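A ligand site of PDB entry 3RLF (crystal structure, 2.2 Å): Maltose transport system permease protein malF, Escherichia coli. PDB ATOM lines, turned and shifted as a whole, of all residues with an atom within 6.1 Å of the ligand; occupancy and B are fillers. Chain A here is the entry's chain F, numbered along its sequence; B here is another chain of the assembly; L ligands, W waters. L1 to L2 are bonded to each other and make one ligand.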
ATOM      1  N   THR A 291       3.410 -11.990  -3.408  1.00  0.00           N
ATOM      2  CA  THR A 291       2.262 -11.787  -2.519  1.00  0.00           C
ATOM      3  C   THR A 291       2.392 -12.681  -1.288  1.00  0.00           C
ATOM      4  O   THR A 291       2.385 -12.182  -0.154  1.00  0.00           O
ATOM      5  CB  THR A 291       0.912 -12.065  -3.228  1.00  0.00           C
ATOM      6  OG1 THR A 291       0.700 -11.098  -4.264  1.00  0.00           O
ATOM      7  CG2 THR A 291      -0.258 -11.987  -2.238  1.00  0.00           C
ATOM      8  N   VAL A 292       2.525 -13.985  -1.524  1.00  0.00           N
ATOM      9  CA  VAL A 292       2.610 -14.971  -0.437  1.00  0.00           C
ATOM     10  C   VAL A 292       3.770 -14.659   0.507  1.00  0.00           C
ATOM     11  O   VAL A 292       3.619 -14.716   1.719  1.00  0.00           O
ATOM     12  CB  VAL A 292       2.698 -16.421  -0.988  1.00  0.00           C
ATOM     13  CG1 VAL A 292       2.955 -17.430   0.132  1.00  0.00           C
ATOM     14  CG2 VAL A 292       1.420 -16.783  -1.735  1.00  0.00           C
ATOM     15  N   THR A 295       2.981 -11.185   2.438  1.00  0.00           N
ATOM     16  CA  THR A 295       1.817 -11.308   3.339  1.00  0.00           C
ATOM     17  C   THR A 295       2.108 -12.195   4.551  1.00  0.00           C
ATOM     18  O   THR A 295       1.671 -11.883   5.658  1.00  0.00           O
ATOM     19  CB  THR A 295       0.550 -11.799   2.607  1.00  0.00           C
ATOM     20  OG1 THR A 295       0.818 -13.032   1.911  1.00  0.00           O
ATOM     21  CG2 THR A 295       0.057 -10.750   1.613  1.00  0.00           C
ATOM     22  N   TYR A 325      -9.353  -6.323   6.348  1.00  0.00           N
ATOM     23  CA  TYR A 325     -10.010  -7.577   6.002  1.00  0.00           C
ATOM     24  C   TYR A 325     -11.479  -7.551   6.461  1.00  0.00           C
ATOM     25  O   TYR A 325     -12.256  -8.430   6.087  1.00  0.00           O
ATOM     26  CB  TYR A 325      -9.248  -8.726   6.658  1.00  0.00           C
ATOM     27  CG  TYR A 325      -9.410 -10.095   6.032  1.00  0.00           C
ATOM     28  CD1 TYR A 325      -9.853 -10.250   4.717  1.00  0.00           C
ATOM     29  CD2 TYR A 325      -9.071 -11.240   6.745  1.00  0.00           C
ATOM     30  CE1 TYR A 325      -9.991 -11.523   4.155  1.00  0.00           C
ATOM     31  CE2 TYR A 325      -9.180 -12.501   6.188  1.00  0.00           C
ATOM     32  CZ  TYR A 325      -9.642 -12.641   4.898  1.00  0.00           C
ATOM     33  OH  TYR A 325      -9.757 -13.898   4.360  1.00  0.00           O
ATOM     34  N   SER A 329     -13.508  -6.210  -0.022  1.00  0.00           N
ATOM     35  CA  SER A 329     -12.354  -5.791  -0.819  1.00  0.00           C
ATOM     36  C   SER A 329     -12.716  -4.980  -2.081  1.00  0.00           C
ATOM     37  O   SER A 329     -11.884  -4.241  -2.596  1.00  0.00           O
ATOM     38  CB  SER A 329     -11.488  -7.003  -1.188  1.00  0.00           C
ATOM     39  OG  SER A 329     -12.158  -7.875  -2.081  1.00  0.00           O
ATOM     40  N   ILE A 333     -10.356  -1.821  -3.252  1.00  0.00           N
ATOM     41  CA  ILE A 333      -9.607  -1.868  -4.516  1.00  0.00           C
ATOM     42  C   ILE A 333      -9.871  -0.612  -5.365  1.00  0.00           C
ATOM     43  O   ILE A 333      -8.938  -0.043  -5.947  1.00  0.00           O
ATOM     44  CB  ILE A 333      -9.893  -3.169  -5.328  1.00  0.00           C
ATOM     45  CG1 ILE A 333      -9.521  -4.403  -4.505  1.00  0.00           C
ATOM     46  CG2 ILE A 333      -9.114  -3.173  -6.644  1.00  0.00           C
ATOM     47  CD1 ILE A 333     -10.023  -5.715  -5.092  1.00  0.00           C
ATOM     48  N   ASN A 376      -2.203  -5.824  -2.924  1.00  0.00           N
ATOM     49  CA  ASN A 376      -2.423  -7.221  -2.581  1.00  0.00           C
ATOM     50  C   ASN A 376      -1.847  -7.600  -1.217  1.00  0.00           C
ATOM     51  O   ASN A 376      -2.381  -8.458  -0.522  1.00  0.00           O
ATOM     52  CB  ASN A 376      -1.870  -8.143  -3.661  1.00  0.00           C
ATOM     53  CG  ASN A 376      -2.694  -9.407  -3.843  1.00  0.00           C
ATOM     54  OD1 ASN A 376      -3.858  -9.464  -3.440  1.00  0.00           O
ATOM     55  ND2 ASN A 376      -2.105 -10.412  -4.476  1.00  0.00           N
ATOM     56  N   THR A 377      -0.745  -6.943  -0.837  1.00  0.00           N
ATOM     57  CA  THR A 377      -0.166  -7.103   0.498  1.00  0.00           C
ATOM     58  C   THR A 377      -1.093  -6.515   1.563  1.00  0.00           C
ATOM     59  O   THR A 377      -1.318  -7.142   2.602  1.00  0.00           O
ATOM     60  CB  THR A 377       1.258  -6.473   0.585  1.00  0.00           C
ATOM     61  OG1 THR A 377       2.125  -7.131  -0.346  1.00  0.00           O
ATOM     62  CG2 THR A 377       1.839  -6.620   1.983  1.00  0.00           C
ATOM     63  N   LEU A 379      -4.327  -6.104   1.286  1.00  0.00           N
ATOM     64  CA  LEU A 379      -5.488  -6.984   1.298  1.00  0.00           C
ATOM     65  C   LEU A 379      -5.207  -8.325   1.966  1.00  0.00           C
ATOM     66  O   LEU A 379      -6.065  -8.889   2.653  1.00  0.00           O
ATOM     67  CB  LEU A 379      -5.983  -7.235  -0.130  1.00  0.00           C
ATOM     68  CG  LEU A 379      -6.656  -6.122  -0.945  1.00  0.00           C
ATOM     69  CD1 LEU A 379      -6.669  -6.483  -2.415  1.00  0.00           C
ATOM     70  CD2 LEU A 379      -8.063  -5.857  -0.437  1.00  0.00           C
ATOM     71  N   GLY A 380      -3.987  -8.829   1.753  1.00  0.00           N
ATOM     72  CA  GLY A 380      -3.639 -10.207   2.109  1.00  0.00           C
ATOM     73  C   GLY A 380      -3.013 -10.462   3.464  1.00  0.00           C
ATOM     74  O   GLY A 380      -3.205 -11.547   4.035  1.00  0.00           O
ATOM     75  N   TYR A 381      -2.268  -9.493   3.992  1.00  0.00           N
ATOM     76  CA  TYR A 381      -1.543  -9.677   5.258  1.00  0.00           C
ATOM     77  C   TYR A 381      -2.415 -10.068   6.470  1.00  0.00           C
ATOM     78  O   TYR A 381      -1.977 -10.879   7.289  1.00  0.00           O
ATOM     79  CB  TYR A 381      -0.603  -8.481   5.580  1.00  0.00           C
ATOM     80  CG  TYR A 381      -1.261  -7.316   6.323  1.00  0.00           C
ATOM     81  CD1 TYR A 381      -1.589  -7.419   7.672  1.00  0.00           C
ATOM     82  CD2 TYR A 381      -1.536  -6.125   5.663  1.00  0.00           C
ATOM     83  CE1 TYR A 381      -2.203  -6.377   8.345  1.00  0.00           C
ATOM     84  CE2 TYR A 381      -2.145  -5.061   6.343  1.00  0.00           C
ATOM     85  CZ  TYR A 381      -2.475  -5.198   7.676  1.00  0.00           C
ATOM     86  OH  TYR A 381      -3.072  -4.172   8.367  1.00  0.00           O
ATOM     87  N   TYR A 383      -5.145 -11.925   6.700  1.00  0.00           N
ATOM     88  CA  TYR A 383      -5.431 -13.360   6.609  1.00  0.00           C
ATOM     89  C   TYR A 383      -4.306 -14.175   7.236  1.00  0.00           C
ATOM     90  O   TYR A 383      -4.564 -15.073   8.050  1.00  0.00           O
ATOM     91  CB  TYR A 383      -5.595 -13.753   5.132  1.00  0.00           C
ATOM     92  CG  TYR A 383      -5.677 -15.246   4.888  1.00  0.00           C
ATOM     93  CD1 TYR A 383      -6.838 -15.959   5.177  1.00  0.00           C
ATOM     94  CD2 TYR A 383      -4.601 -15.944   4.362  1.00  0.00           C
ATOM     95  CE1 TYR A 383      -6.929 -17.326   4.951  1.00  0.00           C
ATOM     96  CE2 TYR A 383      -4.670 -17.321   4.133  1.00  0.00           C
ATOM     97  CZ  TYR A 383      -5.838 -17.991   4.433  1.00  0.00           C
ATOM     98  OH  TYR A 383      -5.931 -19.339   4.203  1.00  0.00           O
ATOM     99  N   MET A 384      -3.073 -13.855   6.849  1.00  0.00           N
ATOM    100  CA  MET A 384      -1.885 -14.538   7.344  1.00  0.00           C
ATOM    101  C   MET A 384      -1.640 -14.203   8.812  1.00  0.00           C
ATOM    102  O   MET A 384      -1.205 -15.055   9.585  1.00  0.00           O
ATOM    103  CB  MET A 384      -0.662 -14.166   6.501  1.00  0.00           C
ATOM    104  CG  MET A 384      -0.675 -14.740   5.089  1.00  0.00           C
ATOM    105  SD  MET A 384      -0.688 -16.544   5.111  1.00  0.00           S
ATOM    106  CE  MET A 384      -0.698 -16.910   3.357  1.00  0.00           C
ATOM    107  N   LEU A 429      -0.859 -23.854   3.617  1.00  0.00           N
ATOM    108  CA  LEU A 429      -1.560 -22.578   3.536  1.00  0.00           C
ATOM    109  C   LEU A 429      -0.894 -21.603   2.563  1.00  0.00           C
ATOM    110  O   LEU A 429      -1.578 -20.853   1.873  1.00  0.00           O
ATOM    111  CB  LEU A 429      -1.713 -21.948   4.922  1.00  0.00           C
ATOM    112  CG  LEU A 429      -2.627 -22.693   5.900  1.00  0.00           C
ATOM    113  CD1 LEU A 429      -2.269 -22.356   7.337  1.00  0.00           C
ATOM    114  CD2 LEU A 429      -4.096 -22.395   5.613  1.00  0.00           C
ATOM    115  N   ALA A 432      -1.725 -23.057  -0.976  1.00  0.00           N
ATOM    116  CA  ALA A 432      -3.087 -22.695  -1.338  1.00  0.00           C
ATOM    117  C   ALA A 432      -3.202 -21.207  -1.678  1.00  0.00           C
ATOM    118  O   ALA A 432      -3.942 -20.830  -2.582  1.00  0.00           O
ATOM    119  CB  ALA A 432      -4.043 -23.048  -0.221  1.00  0.00           C
ATOM    120  N   SER A 433      -2.454 -20.371  -0.946  1.00  0.00           N
ATOM    121  CA  SER A 433      -2.416 -18.940  -1.211  1.00  0.00           C
ATOM    122  C   SER A 433      -1.760 -18.621  -2.557  1.00  0.00           C
ATOM    123  O   SER A 433      -2.166 -17.679  -3.243  1.00  0.00           O
ATOM    124  CB  SER A 433      -1.700 -18.202  -0.080  1.00  0.00           C
ATOM    125  OG  SER A 433      -1.776 -16.792  -0.258  1.00  0.00           O
ATOM    126  N   PHE A 434      -0.746 -19.405  -2.928  1.00  0.00           N
ATOM    127  CA  PHE A 434      -0.126 -19.277  -4.250  1.00  0.00           C
ATOM    128  C   PHE A 434      -1.157 -19.539  -5.345  1.00  0.00           C
ATOM    129  O   PHE A 434      -1.277 -18.762  -6.289  1.00  0.00           O
ATOM    130  CB  PHE A 434       1.074 -20.218  -4.391  1.00  0.00           C
ATOM    131  CG  PHE A 434       1.623 -20.275  -5.796  1.00  0.00           C
ATOM    132  CD1 PHE A 434       1.245 -21.297  -6.663  1.00  0.00           C
ATOM    133  CD2 PHE A 434       2.507 -19.307  -6.252  1.00  0.00           C
ATOM    134  CE1 PHE A 434       1.743 -21.345  -7.957  1.00  0.00           C
ATOM    135  CE2 PHE A 434       3.001 -19.344  -7.539  1.00  0.00           C
ATOM    136  CZ  PHE A 434       2.624 -20.375  -8.404  1.00  0.00           C
ATOM    137  N   PHE A 436      -4.438 -19.450  -5.113  1.00  0.00           N
ATOM    138  CA  PHE A 436      -5.486 -18.437  -5.068  1.00  0.00           C
ATOM    139  C   PHE A 436      -5.075 -17.181  -5.828  1.00  0.00           C
ATOM    140  O   PHE A 436      -5.847 -16.655  -6.640  1.00  0.00           O
ATOM    141  CB  PHE A 436      -5.851 -18.084  -3.621  1.00  0.00           C
ATOM    142  CG  PHE A 436      -6.868 -16.982  -3.497  1.00  0.00           C
ATOM    143  CD1 PHE A 436      -6.482 -15.649  -3.497  1.00  0.00           C
ATOM    144  CD2 PHE A 436      -8.230 -17.290  -3.371  1.00  0.00           C
ATOM    145  CE1 PHE A 436      -7.425 -14.626  -3.380  1.00  0.00           C
ATOM    146  CE2 PHE A 436      -9.172 -16.276  -3.252  1.00  0.00           C
ATOM    147  CZ  PHE A 436      -8.775 -14.934  -3.261  1.00  0.00           C
ATOM    148  N   ASN A 437      -3.865 -16.690  -5.545  1.00  0.00           N
ATOM    149  CA  ASN A 437      -3.341 -15.487  -6.199  1.00  0.00           C
ATOM    150  C   ASN A 437      -2.955 -15.710  -7.664  1.00  0.00           C
ATOM    151  O   ASN A 437      -2.920 -14.748  -8.448  1.00  0.00           O
ATOM    152  CB  ASN A 437      -2.160 -14.919  -5.411  1.00  0.00           C
ATOM    153  CG  ASN A 437      -2.593 -14.245  -4.125  1.00  0.00           C
ATOM    154  OD1 ASN A 437      -2.327 -14.748  -3.030  1.00  0.00           O
ATOM    155  ND2 ASN A 437      -3.276 -13.118  -4.248  1.00  0.00           N
ATOM    156  N   ASN A 440      -6.118 -14.622  -9.402  1.00  0.00           N
ATOM    157  CA  ASN A 440      -6.703 -13.417  -8.793  1.00  0.00           C
ATOM    158  C   ASN A 440      -7.267 -12.453  -9.834  1.00  0.00           C
ATOM    159  O   ASN A 440      -6.843 -11.302  -9.938  1.00  0.00           O
ATOM    160  CB  ASN A 440      -5.693 -12.724  -7.886  1.00  0.00           C
ATOM    161  CG  ASN A 440      -6.322 -12.145  -6.608  1.00  0.00           C
ATOM    162  OD1 ASN A 440      -5.623 -11.907  -5.625  1.00  0.00           O
ATOM    163  ND2 ASN A 440      -7.634 -11.937  -6.622  1.00  0.00           N
ATOM    164  N   LEU A 443      -8.782  -8.558  -8.641  1.00  0.00           N
ATOM    165  CA  LEU A 443      -7.869  -7.458  -8.331  1.00  0.00           C
ATOM    166  C   LEU A 443      -7.280  -6.797  -9.578  1.00  0.00           C
ATOM    167  O   LEU A 443      -7.168  -5.576  -9.636  1.00  0.00           O
ATOM    168  CB  LEU A 443      -6.754  -7.925  -7.388  1.00  0.00           C
ATOM    169  CG  LEU A 443      -5.681  -6.907  -6.975  1.00  0.00           C
ATOM    170  CD1 LEU A 443      -6.277  -5.691  -6.255  1.00  0.00           C
ATOM    171  CD2 LEU A 443      -4.636  -7.569  -6.113  1.00  0.00           C
ATOM    172  N   LEU B 172      -8.989 -26.618   3.402  1.00  0.00           N
ATOM    173  CA  LEU B 172      -7.884 -25.848   3.996  1.00  0.00           C
ATOM    174  C   LEU B 172      -7.952 -25.807   5.521  1.00  0.00           C
ATOM    175  O   LEU B 172      -6.917 -25.882   6.202  1.00  0.00           O
ATOM    176  CB  LEU B 172      -7.861 -24.433   3.444  1.00  0.00           C
ATOM    177  CG  LEU B 172      -6.929 -24.176   2.263  1.00  0.00           C
ATOM    178  CD1 LEU B 172      -7.109 -22.753   1.768  1.00  0.00           C
ATOM    179  CD2 LEU B 172      -5.478 -24.446   2.645  1.00  0.00           C
ATOM    180  N   LEU B 221     -12.075 -16.792  10.246  1.00  0.00           N
ATOM    181  CA  LEU B 221     -11.856 -16.777   8.796  1.00  0.00           C
ATOM    182  C   LEU B 221     -13.098 -17.157   7.999  1.00  0.00           C
ATOM    183  O   LEU B 221     -13.334 -16.597   6.924  1.00  0.00           O
ATOM    184  CB  LEU B 221     -10.678 -17.675   8.409  1.00  0.00           C
ATOM    185  CG  LEU B 221      -9.263 -17.286   8.832  1.00  0.00           C
ATOM    186  CD1 LEU B 221      -8.295 -18.399   8.464  1.00  0.00           C
ATOM    187  CD2 LEU B 221      -8.820 -15.957   8.227  1.00  0.00           C
ATOM    188  N   ALA B 225     -15.296 -14.672   5.467  1.00  0.00           N
ATOM    189  CA  ALA B 225     -15.608 -15.123   4.105  1.00  0.00           C
ATOM    190  C   ALA B 225     -17.109 -15.101   3.827  1.00  0.00           C
ATOM    191  O   ALA B 225     -17.524 -14.742   2.725  1.00  0.00           O
ATOM    192  CB  ALA B 225     -15.033 -16.524   3.855  1.00  0.00           C
HETATM  193  C1  LIG L   1      -8.578 -17.628   1.467  1.00  0.00           C
HETATM  194  C2  LIG L   1      -9.412 -16.461   2.012  1.00  0.00           C
HETATM  195  C3  LIG L   1      -9.215 -15.201   1.190  1.00  0.00           C
HETATM  196  C4  LIG L   1      -7.740 -14.840   1.086  1.00  0.00           C
HETATM  197  C5  LIG L   1      -6.948 -16.015   0.510  1.00  0.00           C
HETATM  198  C6  LIG L   1      -5.456 -15.745   0.617  1.00  0.00           C
HETATM  199  O1  LIG L   1      -9.214 -18.201   0.319  1.00  0.00           O
HETATM  200  O2  LIG L   1     -10.800 -16.824   2.025  1.00  0.00           O
HETATM  201  O3  LIG L   1      -9.933 -14.104   1.759  1.00  0.00           O
HETATM  202  O4  LIG L   1      -7.595 -13.700   0.239  1.00  0.00           O
HETATM  203  O5  LIG L   1      -7.218 -17.261   1.171  1.00  0.00           O
HETATM  204  O6  LIG L   1      -4.735 -16.794  -0.023  1.00  0.00           O
HETATM  205  C1  LG2 L   2      -7.069 -12.539   0.880  1.00  0.00           C
HETATM  206  C2  LG2 L   2      -7.891 -11.318   0.458  1.00  0.00           C
HETATM  207  C3  LG2 L   2      -7.699 -11.013  -1.019  1.00  0.00           C
HETATM  208  C4  LG2 L   2      -6.212 -10.885  -1.374  1.00  0.00           C
HETATM  209  C5  LG2 L   2      -5.424 -12.103  -0.866  1.00  0.00           C
HETATM  210  C6  LG2 L   2      -3.931 -11.906  -1.083  1.00  0.00           C
HETATM  211  O1  LG2 L   2      -9.271 -11.556   0.736  1.00  0.00           O
HETATM  212  O2  LG2 L   2      -8.388  -9.805  -1.348  1.00  0.00           O
HETATM  213  O3  LG2 L   2      -6.068 -10.746  -2.793  1.00  0.00           O
HETATM  214  O4  LG2 L   2      -5.694 -12.347   0.524  1.00  0.00           O
HETATM  215  O5  LG2 L   2      -3.218 -13.121  -0.799  1.00  0.00           O
HETATM  216  O   HOH W   1     -11.482 -15.806   5.142  1.00  0.00           O
HETATM  217  O   HOH W   2      -3.026 -13.620   2.365  1.00  0.00           O
HETATM  218  O   HOH W   3     -10.258  -9.067   1.466  1.00  0.00           O
HETATM  219  O   HOH W   4      -5.667 -19.354   0.143  1.00  0.00           O
HETATM  220  O   HOH W   5      -8.377  -9.772  -4.560  1.00  0.00           O
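O6 of LIG L1 is in hydrogen-bond range of OG of Ser 433 (3.0 Å).
The side-chain amide oxygen (OD1) of Asn 376 is in hydrogen-bond range of an oxygen (O3) of LG2 L2 (2.6 Å).
The side-chain amide oxygen (OD1) of Asn 440 sits at hydrogen-bond distance from an oxygen (O3) of LG2 L2 (3.1 Å).
The side-chain hydroxyl (OH) of Tyr 325 is in hydrogen-bond range of an oxygen (O3) of LIG L1.
OD1 of Asn 437 lies within hydrogen-bond range of O5 of LG2 L2.
The side-chain amide oxygen (OD1) of Asn 437 lies close to the backbone carbonyl oxygen (O) of Ser 433 (2.9 Å).
The side-chain amide nitrogen (ND2) of Asn 437 lies close to the side-chain amide nitrogen (ND2) of Asn 376 (3.0 Å).
The side-chain amide nitrogen of Asn 437 is in hydrogen-bond range of the side-chain amide oxygen of Asn 440 (3.0 Å).
The side-chain amide nitrogen (ND2) of Asn 376 lies within hydrogen-bond range of the side-chain hydroxyl (OG1) of Thr 291 (2.9 Å).
The side-chain hydroxyl (OG1) of Thr 295 is in hydrogen-bond range of the backbone carbonyl oxygen (O) of Thr 291 (2.7 Å).
CG2 of Thr 291 touches O5 of LG2 L2, 3.5 Å away.
CB of Leu 379 touches O2 of LG2 L2 (3.7 Å).
CA of Gly 380 touches O4 of LG2 L2, at 3.4 Å.
CZ of Tyr 383 touches O5 of LIG L1, at 3.6 Å.
CE1 of Phe 436 touches O4 of LIG L1 (3.7 Å).
Hydrophobic or aromatic side chains within 4 Å of the ligand: Tyr 325, Leu 379, Tyr 383 and Phe 436.
Within 4 Å of the ligand: Thr 291, Tyr 325, Asn 376, Leu 379, Gly 380, Tyr 383, Ser 433, Phe 436, Asn 437 and Asn 440.
Water W5 lies within hydrogen-bond range of an oxygen (O3) of LG2 L2 (3.1 Å) and the side-chain amide nitrogen of Asn 440 (3.1 Å).
Water W2 bridges O of Gly 380 (2.7 Å) and O5 of LG2 L2 (3.2 Å).
Water W1 lies within hydrogen-bond range of the side-chain hydroxyl of Tyr 325, the backbone carbonyl oxygen of Leu 221 of chain B and an oxygen (O2) of LIG L1.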
